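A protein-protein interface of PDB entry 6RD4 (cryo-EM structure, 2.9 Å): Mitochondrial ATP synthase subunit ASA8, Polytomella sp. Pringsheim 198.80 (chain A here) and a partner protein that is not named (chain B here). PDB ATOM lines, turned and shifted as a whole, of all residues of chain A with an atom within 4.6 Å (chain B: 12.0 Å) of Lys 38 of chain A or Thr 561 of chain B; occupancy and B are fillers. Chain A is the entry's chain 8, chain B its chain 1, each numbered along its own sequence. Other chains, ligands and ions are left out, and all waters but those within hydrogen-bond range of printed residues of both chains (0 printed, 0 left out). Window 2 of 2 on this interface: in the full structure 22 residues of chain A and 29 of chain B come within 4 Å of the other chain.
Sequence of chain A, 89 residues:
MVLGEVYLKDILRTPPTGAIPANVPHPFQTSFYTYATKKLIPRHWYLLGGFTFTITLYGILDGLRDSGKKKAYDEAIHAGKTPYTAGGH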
ATOM      1  N   HIS A  26     -36.350  15.129   5.333  1.00  0.00           N
ATOM      2  CA  HIS A  26     -35.029  14.573   5.318  1.00  0.00           C
ATOM      3  C   HIS A  26     -34.855  13.764   4.037  1.00  0.00           C
ATOM      4  O   HIS A  26     -35.836  13.304   3.459  1.00  0.00           O
ATOM      5  CB  HIS A  26     -34.822  13.697   6.536  1.00  0.00           C
ATOM      6  CG  HIS A  26     -33.408  13.307   6.744  1.00  0.00           C
ATOM      7  ND1 HIS A  26     -32.501  14.119   7.363  1.00  0.00           N
ATOM      8  CD2 HIS A  26     -32.725  12.222   6.344  1.00  0.00           C
ATOM      9  CE1 HIS A  26     -31.324  13.531   7.366  1.00  0.00           C
ATOM     10  NE2 HIS A  26     -31.434  12.378   6.748  1.00  0.00           N
ATOM     11  N   PRO A  27     -33.626  13.611   3.544  1.00  0.00           N
ATOM     12  CA  PRO A  27     -33.397  12.719   2.404  1.00  0.00           C
ATOM     13  C   PRO A  27     -33.799  11.274   2.616  1.00  0.00           C
ATOM     14  O   PRO A  27     -34.002  10.568   1.633  1.00  0.00           O
ATOM     15  CB  PRO A  27     -31.898  12.845   2.195  1.00  0.00           C
ATOM     16  CG  PRO A  27     -31.641  14.212   2.542  1.00  0.00           C
ATOM     17  CD  PRO A  27     -32.537  14.584   3.653  1.00  0.00           C
ATOM     18  N   PHE A  28     -33.925  10.814   3.851  1.00  0.00           N
ATOM     19  CA  PHE A  28     -34.348   9.462   4.157  1.00  0.00           C
ATOM     20  C   PHE A  28     -35.854   9.336   4.141  1.00  0.00           C
ATOM     21  O   PHE A  28     -36.377   8.264   3.854  1.00  0.00           O
ATOM     22  CB  PHE A  28     -33.850   9.053   5.530  1.00  0.00           C
ATOM     23  CG  PHE A  28     -32.377   8.876   5.632  1.00  0.00           C
ATOM     24  CD1 PHE A  28     -31.583   8.778   4.524  1.00  0.00           C
ATOM     25  CD2 PHE A  28     -31.796   8.748   6.859  1.00  0.00           C
ATOM     26  CE1 PHE A  28     -30.258   8.598   4.647  1.00  0.00           C
ATOM     27  CE2 PHE A  28     -30.476   8.562   6.968  1.00  0.00           C
ATOM     28  CZ  PHE A  28     -29.715   8.476   5.862  1.00  0.00           C
ATOM     29  N   THR A  34     -32.319   6.076  -0.691  1.00  0.00           N
ATOM     30  CA  THR A  34     -31.260   6.830  -0.037  1.00  0.00           C
ATOM     31  C   THR A  34     -31.014   6.308   1.359  1.00  0.00           C
ATOM     32  O   THR A  34     -29.877   6.299   1.818  1.00  0.00           O
ATOM     33  CB  THR A  34     -31.621   8.300   0.038  1.00  0.00           C
ATOM     34  OG1 THR A  34     -32.180   8.698  -1.212  1.00  0.00           O
ATOM     35  CG2 THR A  34     -30.410   9.127   0.289  1.00  0.00           C
ATOM     36  N   TYR A  35     -32.067   5.873   2.047  1.00  0.00           N
ATOM     37  CA  TYR A  35     -31.890   5.268   3.351  1.00  0.00           C
ATOM     38  C   TYR A  35     -31.170   3.950   3.233  1.00  0.00           C
ATOM     39  O   TYR A  35     -30.266   3.670   4.019  1.00  0.00           O
ATOM     40  CB  TYR A  35     -33.227   5.052   4.030  1.00  0.00           C
ATOM     41  CG  TYR A  35     -33.083   4.324   5.330  1.00  0.00           C
ATOM     42  CD1 TYR A  35     -32.256   4.810   6.305  1.00  0.00           C
ATOM     43  CD2 TYR A  35     -33.758   3.158   5.576  1.00  0.00           C
ATOM     44  CE1 TYR A  35     -32.096   4.173   7.444  1.00  0.00           C
ATOM     45  CE2 TYR A  35     -33.605   2.516   6.753  1.00  0.00           C
ATOM     46  CZ  TYR A  35     -32.777   3.037   7.680  1.00  0.00           C
ATOM     47  OH  TYR A  35     -32.582   2.413   8.867  1.00  0.00           O
ATOM     48  N   ALA A  36     -31.562   3.130   2.260  1.00  0.00           N
ATOM     49  CA  ALA A  36     -31.018   1.792   2.141  1.00  0.00           C
ATOM     50  C   ALA A  36     -29.560   1.809   1.778  1.00  0.00           C
ATOM     51  O   ALA A  36     -28.784   1.045   2.336  1.00  0.00           O
ATOM     52  CB  ALA A  36     -31.781   0.996   1.108  1.00  0.00           C
ATOM     53  N   THR A  37     -29.154   2.687   0.890  1.00  0.00           N
ATOM     54  CA  THR A  37     -27.791   2.657   0.411  1.00  0.00           C
ATOM     55  C   THR A  37     -26.839   3.499   1.226  1.00  0.00           C
ATOM     56  O   THR A  37     -25.646   3.211   1.234  1.00  0.00           O
ATOM     57  CB  THR A  37     -27.755   3.101  -1.038  1.00  0.00           C
ATOM     58  OG1 THR A  37     -28.434   4.346  -1.152  1.00  0.00           O
ATOM     59  CG2 THR A  37     -28.489   2.107  -1.855  1.00  0.00           C
ATOM     60  N   LYS A  38     -27.323   4.520   1.922  1.00  0.00           N
ATOM     61  CA  LYS A  38     -26.457   5.338   2.752  1.00  0.00           C
ATOM     62  C   LYS A  38     -26.523   4.996   4.223  1.00  0.00           C
ATOM     63  O   LYS A  38     -25.581   5.313   4.947  1.00  0.00           O
ATOM     64  CB  LYS A  38     -26.794   6.815   2.599  1.00  0.00           C
ATOM     65  CG  LYS A  38     -26.600   7.339   1.226  1.00  0.00           C
ATOM     66  CD  LYS A  38     -26.335   8.815   1.247  1.00  0.00           C
ATOM     67  CE  LYS A  38     -26.180   9.332  -0.164  1.00  0.00           C
ATOM     68  NZ  LYS A  38     -25.760  10.754  -0.207  1.00  0.00           N
ATOM     69  N   LYS A  39     -27.581   4.407   4.685  1.00  0.00           N
ATOM     70  CA  LYS A  39     -27.567   4.110   6.101  1.00  0.00           C
ATOM     71  C   LYS A  39     -27.892   2.673   6.428  1.00  0.00           C
ATOM     72  O   LYS A  39     -27.224   2.095   7.266  1.00  0.00           O
ATOM     73  CB  LYS A  39     -28.525   5.001   6.831  1.00  0.00           C
ATOM     74  CG  LYS A  39     -28.519   4.802   8.296  1.00  0.00           C
ATOM     75  CD  LYS A  39     -29.123   5.935   8.959  1.00  0.00           C
ATOM     76  CE  LYS A  39     -28.112   6.922   9.304  1.00  0.00           C
ATOM     77  NZ  LYS A  39     -27.315   6.387  10.388  1.00  0.00           N
ATOM     78  N   LEU A  40     -28.875   2.074   5.775  1.00  0.00           N
ATOM     79  CA  LEU A  40     -29.324   0.754   6.182  1.00  0.00           C
ATOM     80  C   LEU A  40     -28.298  -0.311   5.857  1.00  0.00           C
ATOM     81  O   LEU A  40     -28.035  -1.191   6.671  1.00  0.00           O
ATOM     82  CB  LEU A  40     -30.650   0.435   5.521  1.00  0.00           C
ATOM     83  CG  LEU A  40     -31.251  -0.936   5.677  1.00  0.00           C
ATOM     84  CD1 LEU A  40     -31.531  -1.200   7.112  1.00  0.00           C
ATOM     85  CD2 LEU A  40     -32.510  -0.975   4.896  1.00  0.00           C
ATOM     86  N   PRO A  42     -24.770   0.317   4.792  1.00  0.00           N
ATOM     87  CA  PRO A  42     -23.455   0.528   5.404  1.00  0.00           C
ATOM     88  C   PRO A  42     -23.420   0.419   6.909  1.00  0.00           C
ATOM     89  O   PRO A  42     -22.393   0.006   7.452  1.00  0.00           O
ATOM     90  CB  PRO A  42     -23.093   1.938   4.953  1.00  0.00           C
ATOM     91  CG  PRO A  42     -23.784   2.089   3.762  1.00  0.00           C
ATOM     92  CD  PRO A  42     -25.081   1.485   3.962  1.00  0.00           C
ATOM     93  N   LEU B 552     -29.283  25.645   8.453  1.00  0.00           N
ATOM     94  CA  LEU B 552     -28.998  24.935   9.687  1.00  0.00           C
ATOM     95  C   LEU B 552     -29.615  23.564   9.649  1.00  0.00           C
ATOM     96  O   LEU B 552     -28.995  22.586  10.054  1.00  0.00           O
ATOM     97  CB  LEU B 552     -29.527  25.700  10.884  1.00  0.00           C
ATOM     98  CG  LEU B 552     -29.309  25.034  12.224  1.00  0.00           C
ATOM     99  CD1 LEU B 552     -27.867  24.939  12.519  1.00  0.00           C
ATOM    100  CD2 LEU B 552     -29.985  25.771  13.283  1.00  0.00           C
ATOM    101  N   ILE B 553     -30.835  23.478   9.141  1.00  0.00           N
ATOM    102  CA  ILE B 553     -31.511  22.213   8.926  1.00  0.00           C
ATOM    103  C   ILE B 553     -30.792  21.390   7.878  1.00  0.00           C
ATOM    104  O   ILE B 553     -30.709  20.176   8.000  1.00  0.00           O
ATOM    105  CB  ILE B 553     -32.964  22.526   8.553  1.00  0.00           C
ATOM    106  CG1 ILE B 553     -33.664  23.171   9.733  1.00  0.00           C
ATOM    107  CG2 ILE B 553     -33.698  21.352   8.086  1.00  0.00           C
ATOM    108  CD1 ILE B 553     -33.589  22.405  10.980  1.00  0.00           C
ATOM    109  N   LYS B 554     -30.211  22.029   6.871  1.00  0.00           N
ATOM    110  CA  LYS B 554     -29.456  21.331   5.842  1.00  0.00           C
ATOM    111  C   LYS B 554     -28.198  20.696   6.397  1.00  0.00           C
ATOM    112  O   LYS B 554     -27.836  19.592   6.005  1.00  0.00           O
ATOM    113  CB  LYS B 554     -29.094  22.299   4.731  1.00  0.00           C
ATOM    114  CG  LYS B 554     -28.408  21.684   3.566  1.00  0.00           C
ATOM    115  CD  LYS B 554     -27.566  22.681   2.878  1.00  0.00           C
ATOM    116  CE  LYS B 554     -26.870  22.081   1.728  1.00  0.00           C
ATOM    117  NZ  LYS B 554     -25.886  23.034   1.202  1.00  0.00           N
ATOM    118  N   LYS B 555     -27.520  21.373   7.311  1.00  0.00           N
ATOM    119  CA  LYS B 555     -26.312  20.832   7.908  1.00  0.00           C
ATOM    120  C   LYS B 555     -26.603  19.841   9.013  1.00  0.00           C
ATOM    121  O   LYS B 555     -25.774  18.984   9.286  1.00  0.00           O
ATOM    122  CB  LYS B 555     -25.467  21.948   8.478  1.00  0.00           C
ATOM    123  CG  LYS B 555     -24.920  22.872   7.484  1.00  0.00           C
ATOM    124  CD  LYS B 555     -24.094  23.882   8.155  1.00  0.00           C
ATOM    125  CE  LYS B 555     -24.285  25.192   7.549  1.00  0.00           C
ATOM    126  NZ  LYS B 555     -23.167  26.048   7.888  1.00  0.00           N
ATOM    127  N   ILE B 556     -27.724  19.985   9.708  1.00  0.00           N
ATOM    128  CA  ILE B 556     -28.154  18.985  10.674  1.00  0.00           C
ATOM    129  C   ILE B 556     -28.512  17.694   9.969  1.00  0.00           C
ATOM    130  O   ILE B 556     -28.135  16.609  10.407  1.00  0.00           O
ATOM    131  CB  ILE B 556     -29.331  19.529  11.495  1.00  0.00           C
ATOM    132  CG1 ILE B 556     -28.851  20.476  12.573  1.00  0.00           C
ATOM    133  CG2 ILE B 556     -30.074  18.453  12.143  1.00  0.00           C
ATOM    134  CD1 ILE B 556     -29.938  21.261  13.133  1.00  0.00           C
ATOM    135  N   ASP B 557     -29.206  17.794   8.841  1.00  0.00           N
ATOM    136  CA  ASP B 557     -29.548  16.632   8.041  1.00  0.00           C
ATOM    137  C   ASP B 557     -28.348  15.967   7.422  1.00  0.00           C
ATOM    138  O   ASP B 557     -28.453  14.823   7.005  1.00  0.00           O
ATOM    139  CB  ASP B 557     -30.480  17.019   6.914  1.00  0.00           C
ATOM    140  CG  ASP B 557     -31.834  17.366   7.386  1.00  0.00           C
ATOM    141  OD1 ASP B 557     -32.053  17.352   8.600  1.00  0.00           O
ATOM    142  OD2 ASP B 557     -32.691  17.649   6.539  1.00  0.00           O
ATOM    143  N   TRP B 558     -27.233  16.663   7.286  1.00  0.00           N
ATOM    144  CA  TRP B 558     -26.039  16.010   6.784  1.00  0.00           C
ATOM    145  C   TRP B 558     -25.472  15.065   7.817  1.00  0.00           C
ATOM    146  O   TRP B 558     -24.911  14.034   7.467  1.00  0.00           O
ATOM    147  CB  TRP B 558     -24.993  17.035   6.374  1.00  0.00           C
ATOM    148  CG  TRP B 558     -23.807  16.432   5.735  1.00  0.00           C
ATOM    149  CD1 TRP B 558     -23.627  16.216   4.431  1.00  0.00           C
ATOM    150  CD2 TRP B 558     -22.632  15.954   6.388  1.00  0.00           C
ATOM    151  NE1 TRP B 558     -22.421  15.630   4.215  1.00  0.00           N
ATOM    152  CE2 TRP B 558     -21.793  15.469   5.415  1.00  0.00           C
ATOM    153  CE3 TRP B 558     -22.218  15.894   7.711  1.00  0.00           C
ATOM    154  CZ2 TRP B 558     -20.589  14.915   5.710  1.00  0.00           C
ATOM    155  CZ3 TRP B 558     -21.043  15.356   7.996  1.00  0.00           C
ATOM    156  CH2 TRP B 558     -20.231  14.872   7.015  1.00  0.00           C
ATOM    157  N   GLU B 559     -25.584  15.404   9.088  1.00  0.00           N
ATOM    158  CA  GLU B 559     -25.080  14.519  10.119  1.00  0.00           C
ATOM    159  C   GLU B 559     -25.944  13.284  10.258  1.00  0.00           C
ATOM    160  O   GLU B 559     -25.436  12.207  10.548  1.00  0.00           O
ATOM    161  CB  GLU B 559     -25.019  15.251  11.433  1.00  0.00           C
ATOM    162  CG  GLU B 559     -24.349  16.536  11.339  1.00  0.00           C
ATOM    163  CD  GLU B 559     -23.981  17.067  12.671  1.00  0.00           C
ATOM    164  OE1 GLU B 559     -23.956  16.284  13.621  1.00  0.00           O
ATOM    165  OE2 GLU B 559     -23.725  18.269  12.785  1.00  0.00           O
ATOM    166  N   THR B 560     -27.250  13.418  10.087  1.00  0.00           N
ATOM    167  CA  THR B 560     -28.106  12.247  10.142  1.00  0.00           C
ATOM    168  C   THR B 560     -27.900  11.368   8.926  1.00  0.00           C
ATOM    169  O   THR B 560     -27.902  10.148   9.041  1.00  0.00           O
ATOM    170  CB  THR B 560     -29.561  12.663  10.263  1.00  0.00           C
ATOM    171  OG1 THR B 560     -29.679  13.647  11.283  1.00  0.00           O
ATOM    172  CG2 THR B 560     -30.394  11.525  10.651  1.00  0.00           C
ATOM    173  N   THR B 561     -27.695  11.969   7.762  1.00  0.00           N
ATOM    174  CA  THR B 561     -27.497  11.192   6.548  1.00  0.00           C
ATOM    175  C   THR B 561     -26.179  10.457   6.580  1.00  0.00           C
ATOM    176  O   THR B 561     -26.098   9.289   6.203  1.00  0.00           O
ATOM    177  CB  THR B 561     -27.555  12.108   5.346  1.00  0.00           C
ATOM    178  OG1 THR B 561     -28.793  12.805   5.361  1.00  0.00           O
ATOM    179  CG2 THR B 561     -27.469  11.348   4.091  1.00  0.00           C
ATOM    180  N   ASN B 562     -25.144  11.113   7.072  1.00  0.00           N
ATOM    181  CA  ASN B 562     -23.806  10.558   7.098  1.00  0.00           C
ATOM    182  C   ASN B 562     -23.449   9.983   8.440  1.00  0.00           C
ATOM    183  O   ASN B 562     -22.302  10.091   8.857  1.00  0.00           O
ATOM    184  CB  ASN B 562     -22.812  11.619   6.694  1.00  0.00           C
ATOM    185  CG  ASN B 562     -23.010  12.028   5.302  1.00  0.00           C
ATOM    186  OD1 ASN B 562     -23.828  12.868   5.020  1.00  0.00           O
ATOM    187  ND2 ASN B 562     -22.309  11.399   4.397  1.00  0.00           N
ATOM    188  N   ALA B 563     -24.435   9.437   9.134  1.00  0.00           N
ATOM    189  CA  ALA B 563     -24.281   8.542  10.269  1.00  0.00           C
ATOM    190  C   ALA B 563     -23.560   9.170  11.435  1.00  0.00           C
ATOM    191  O   ALA B 563     -22.953   8.471  12.236  1.00  0.00           O
ATOM    192  CB  ALA B 563     -23.574   7.260   9.853  1.00  0.00           C
ATOM    193  N   LEU B 564     -23.592  10.482  11.540  1.00  0.00           N
ATOM    194  CA  LEU B 564     -22.982  11.202  12.638  1.00  0.00           C
ATOM    195  C   LEU B 564     -24.040  11.906  13.457  1.00  0.00           C
ATOM    196  O   LEU B 564     -23.830  13.011  13.930  1.00  0.00           O
ATOM    197  CB  LEU B 564     -21.981  12.227  12.140  1.00  0.00           C
ATOM    198  CG  LEU B 564     -20.792  11.850  11.289  1.00  0.00           C
ATOM    199  CD1 LEU B 564     -20.316  13.093  10.661  1.00  0.00           C
ATOM    200  CD2 LEU B 564     -19.730  11.303  12.156  1.00  0.00           C
ATOM    201  N   GLU B 565     -25.195  11.271  13.639  1.00  0.00           N
ATOM    202  CA  GLU B 565     -26.267  11.905  14.386  1.00  0.00           C
ATOM    203  C   GLU B 565     -25.965  12.002  15.865  1.00  0.00           C
ATOM    204  O   GLU B 565     -26.684  12.686  16.588  1.00  0.00           O
ATOM    205  CB  GLU B 565     -27.580  11.161  14.190  1.00  0.00           C
ATOM    206  CG  GLU B 565     -27.611   9.811  14.815  1.00  0.00           C
ATOM    207  CD  GLU B 565     -27.231   8.730  13.858  1.00  0.00           C
ATOM    208  OE1 GLU B 565     -26.827   9.057  12.734  1.00  0.00           O
ATOM    209  OE2 GLU B 565     -27.315   7.547  14.225  1.00  0.00           O
ATOM    210  N   ASP B 566     -24.930  11.343  16.340  1.00  0.00           N
ATOM    211  CA  ASP B 566     -24.485  11.483  17.708  1.00  0.00           C
ATOM    212  C   ASP B 566     -23.140  12.178  17.797  1.00  0.00           C
ATOM    213  O   ASP B 566     -22.366  11.886  18.699  1.00  0.00           O
ATOM    214  CB  ASP B 566     -24.403  10.118  18.366  1.00  0.00           C
ATOM    215  CG  ASP B 566     -23.499   9.179  17.628  1.00  0.00           C
ATOM    216  OD1 ASP B 566     -23.464   9.225  16.391  1.00  0.00           O
ATOM    217  OD2 ASP B 566     -22.818   8.379  18.286  1.00  0.00           O
ATOM    218  N   PHE B 567     -22.845  13.098  16.879  1.00  0.00           N
ATOM    219  CA  PHE B 567     -21.508  13.670  16.834  1.00  0.00           C
ATOM    220  C   PHE B 567     -21.243  14.586  18.008  1.00  0.00           C
ATOM    221  O   PHE B 567     -20.114  14.654  18.482  1.00  0.00           O
ATOM    222  CB  PHE B 567     -21.279  14.431  15.541  1.00  0.00           C
ATOM    223  CG  PHE B 567     -19.859  14.837  15.338  1.00  0.00           C
ATOM    224  CD1 PHE B 567     -18.860  13.892  15.310  1.00  0.00           C
ATOM    225  CD2 PHE B 567     -19.521  16.157  15.163  1.00  0.00           C
ATOM    226  CE1 PHE B 567     -17.553  14.258  15.125  1.00  0.00           C
ATOM    227  CE2 PHE B 567     -18.224  16.524  14.980  1.00  0.00           C
ATOM    228  CZ  PHE B 567     -17.240  15.575  14.956  1.00  0.00           C
ATOM    229  N   TRP B 583     -17.889  22.924  16.574  1.00  0.00           N
ATOM    230  CA  TRP B 583     -18.983  22.251  15.894  1.00  0.00           C
ATOM    231  C   TRP B 583     -20.219  23.115  15.882  1.00  0.00           C
ATOM    232  O   TRP B 583     -20.904  23.206  14.866  1.00  0.00           O
ATOM    233  CB  TRP B 583     -19.270  20.916  16.563  1.00  0.00           C
ATOM    234  CG  TRP B 583     -20.574  20.297  16.207  1.00  0.00           C
ATOM    235  CD1 TRP B 583     -20.856  19.568  15.108  1.00  0.00           C
ATOM    236  CD2 TRP B 583     -21.767  20.337  16.972  1.00  0.00           C
ATOM    237  NE1 TRP B 583     -22.149  19.172  15.123  1.00  0.00           N
ATOM    238  CE2 TRP B 583     -22.731  19.637  16.266  1.00  0.00           C
ATOM    239  CE3 TRP B 583     -22.117  20.922  18.181  1.00  0.00           C
ATOM    240  CZ2 TRP B 583     -24.011  19.488  16.729  1.00  0.00           C
ATOM    241  CZ3 TRP B 583     -23.374  20.771  18.630  1.00  0.00           C
ATOM    242  CH2 TRP B 583     -24.307  20.052  17.919  1.00  0.00           C
ATOM    243  N   ASN B 587     -21.802  25.424  12.386  1.00  0.00           N
ATOM    244  CA  ASN B 587     -23.136  25.101  11.928  1.00  0.00           C
ATOM    245  C   ASN B 587     -24.037  26.301  11.890  1.00  0.00           C
ATOM    246  O   ASN B 587     -25.082  26.254  11.246  1.00  0.00           O
ATOM    247  CB  ASN B 587     -23.777  24.051  12.820  1.00  0.00           C
ATOM    248  CG  ASN B 587     -23.387  22.661  12.445  1.00  0.00           C
ATOM    249  OD1 ASN B 587     -23.710  21.718  13.135  1.00  0.00           O
ATOM    250  ND2 ASN B 587     -22.686  22.523  11.347  1.00  0.00           N
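OE1 of Glu 565 of chain B is in salt-bridge range of NZ of Lys 39 of chain A (3.6 Å). OD1 of Asp 557 of chain B sits close to ND1 of His 26 of chain A (3.5 Å). OG1 of Thr 561 of chain B sits at hydrogen-bond distance from NE2 of His 26 of chain A, 3.0 Å away.
The backbone carbonyl oxygen of Glu 559 of chain B lies within hydrogen-bond range of the backbone NH of Glu 565 of chain B (3.2 Å). O of Ile 556 of chain B sits at hydrogen-bond distance from OG1 of Thr 560 of chain B (3.5 Å). O of Asp 557 of chain B is in hydrogen-bond range of OG1 of Thr 561 of chain B (2.6 Å).
Among the printed residues, merely in contact across the chains: Lys 39 of chain A with Thr 560 of chain B (3.2 Å), His 26 of chain A with Thr 560 of chain B (3.5 Å), Phe 28 of chain A with Thr 561 of chain B (3.6 Å), Phe 28 of chain A with Thr 560 of chain B (3.7 Å), Lys 39 of chain A with Ala 563 of chain B (3.7 Å) and Lys 38 of chain A with Thr 561 of chain B (3.97 Å).
His 26 of chain A touches just these residues of chain B: Asp 557, Thr 560 and Thr 561. No residue of chain B comes within 4 Å of Pro 27 of chain A. Of the printed residues of chain B, Phe 28 of chain A touches Thr 560 and Thr 561. No residue of chain B comes within 4 Å of Ala 36 of chain A. No residue of chain B comes within 4 Å of Thr 37 of chain A. Lys 38 of chain A touches one residue of chain B. Of chain B, only Thr 560 (3.2 Å), Ala 563 (3.7 Å) and Glu 565 (3.6 Å) come within 4 Å of Lys 39 of chain A. Ile 553 of chain B touches none of the printed residues of chain A. Of the printed residues of chain A, Asp 557 of chain B touches His 26. Of chain A, only His 26, Phe 28 and Lys 38 come within 4 Å of Thr 561 of chain B. Printed residues of chain A within 4 Å of Ala 563 of chain B: Lys 39 (3.7 Å). Printed residues of chain A within 4 Å of Glu 565 of chain B: Lys 39 (3.6 Å). The nearest residue of chain B that does not touch Lys 38 of chain A is Ala 563 of chain B (5.6 Å). The nearest residue of chain A that does not touch Thr 561 of chain B is Pro 27 of chain A (4.2 Å). The nearest printed residue of chain A that does not touch Asp 557 of chain B is Pro 27 of chain A (4.2 Å).
Hydrophobic or aromatic side chains of chain A that line the printed part of chain B: His 26 and Phe 28. Of the 18 printed residues of chain B, 5 touch a printed residue of chain A. Among the printed residues, Asp or Glu carboxylates within 4 Å of a Lys or Arg side-chain nitrogen of the other chain: Lys 39 of chain A with Glu 565 of chain B (3.6 Å).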
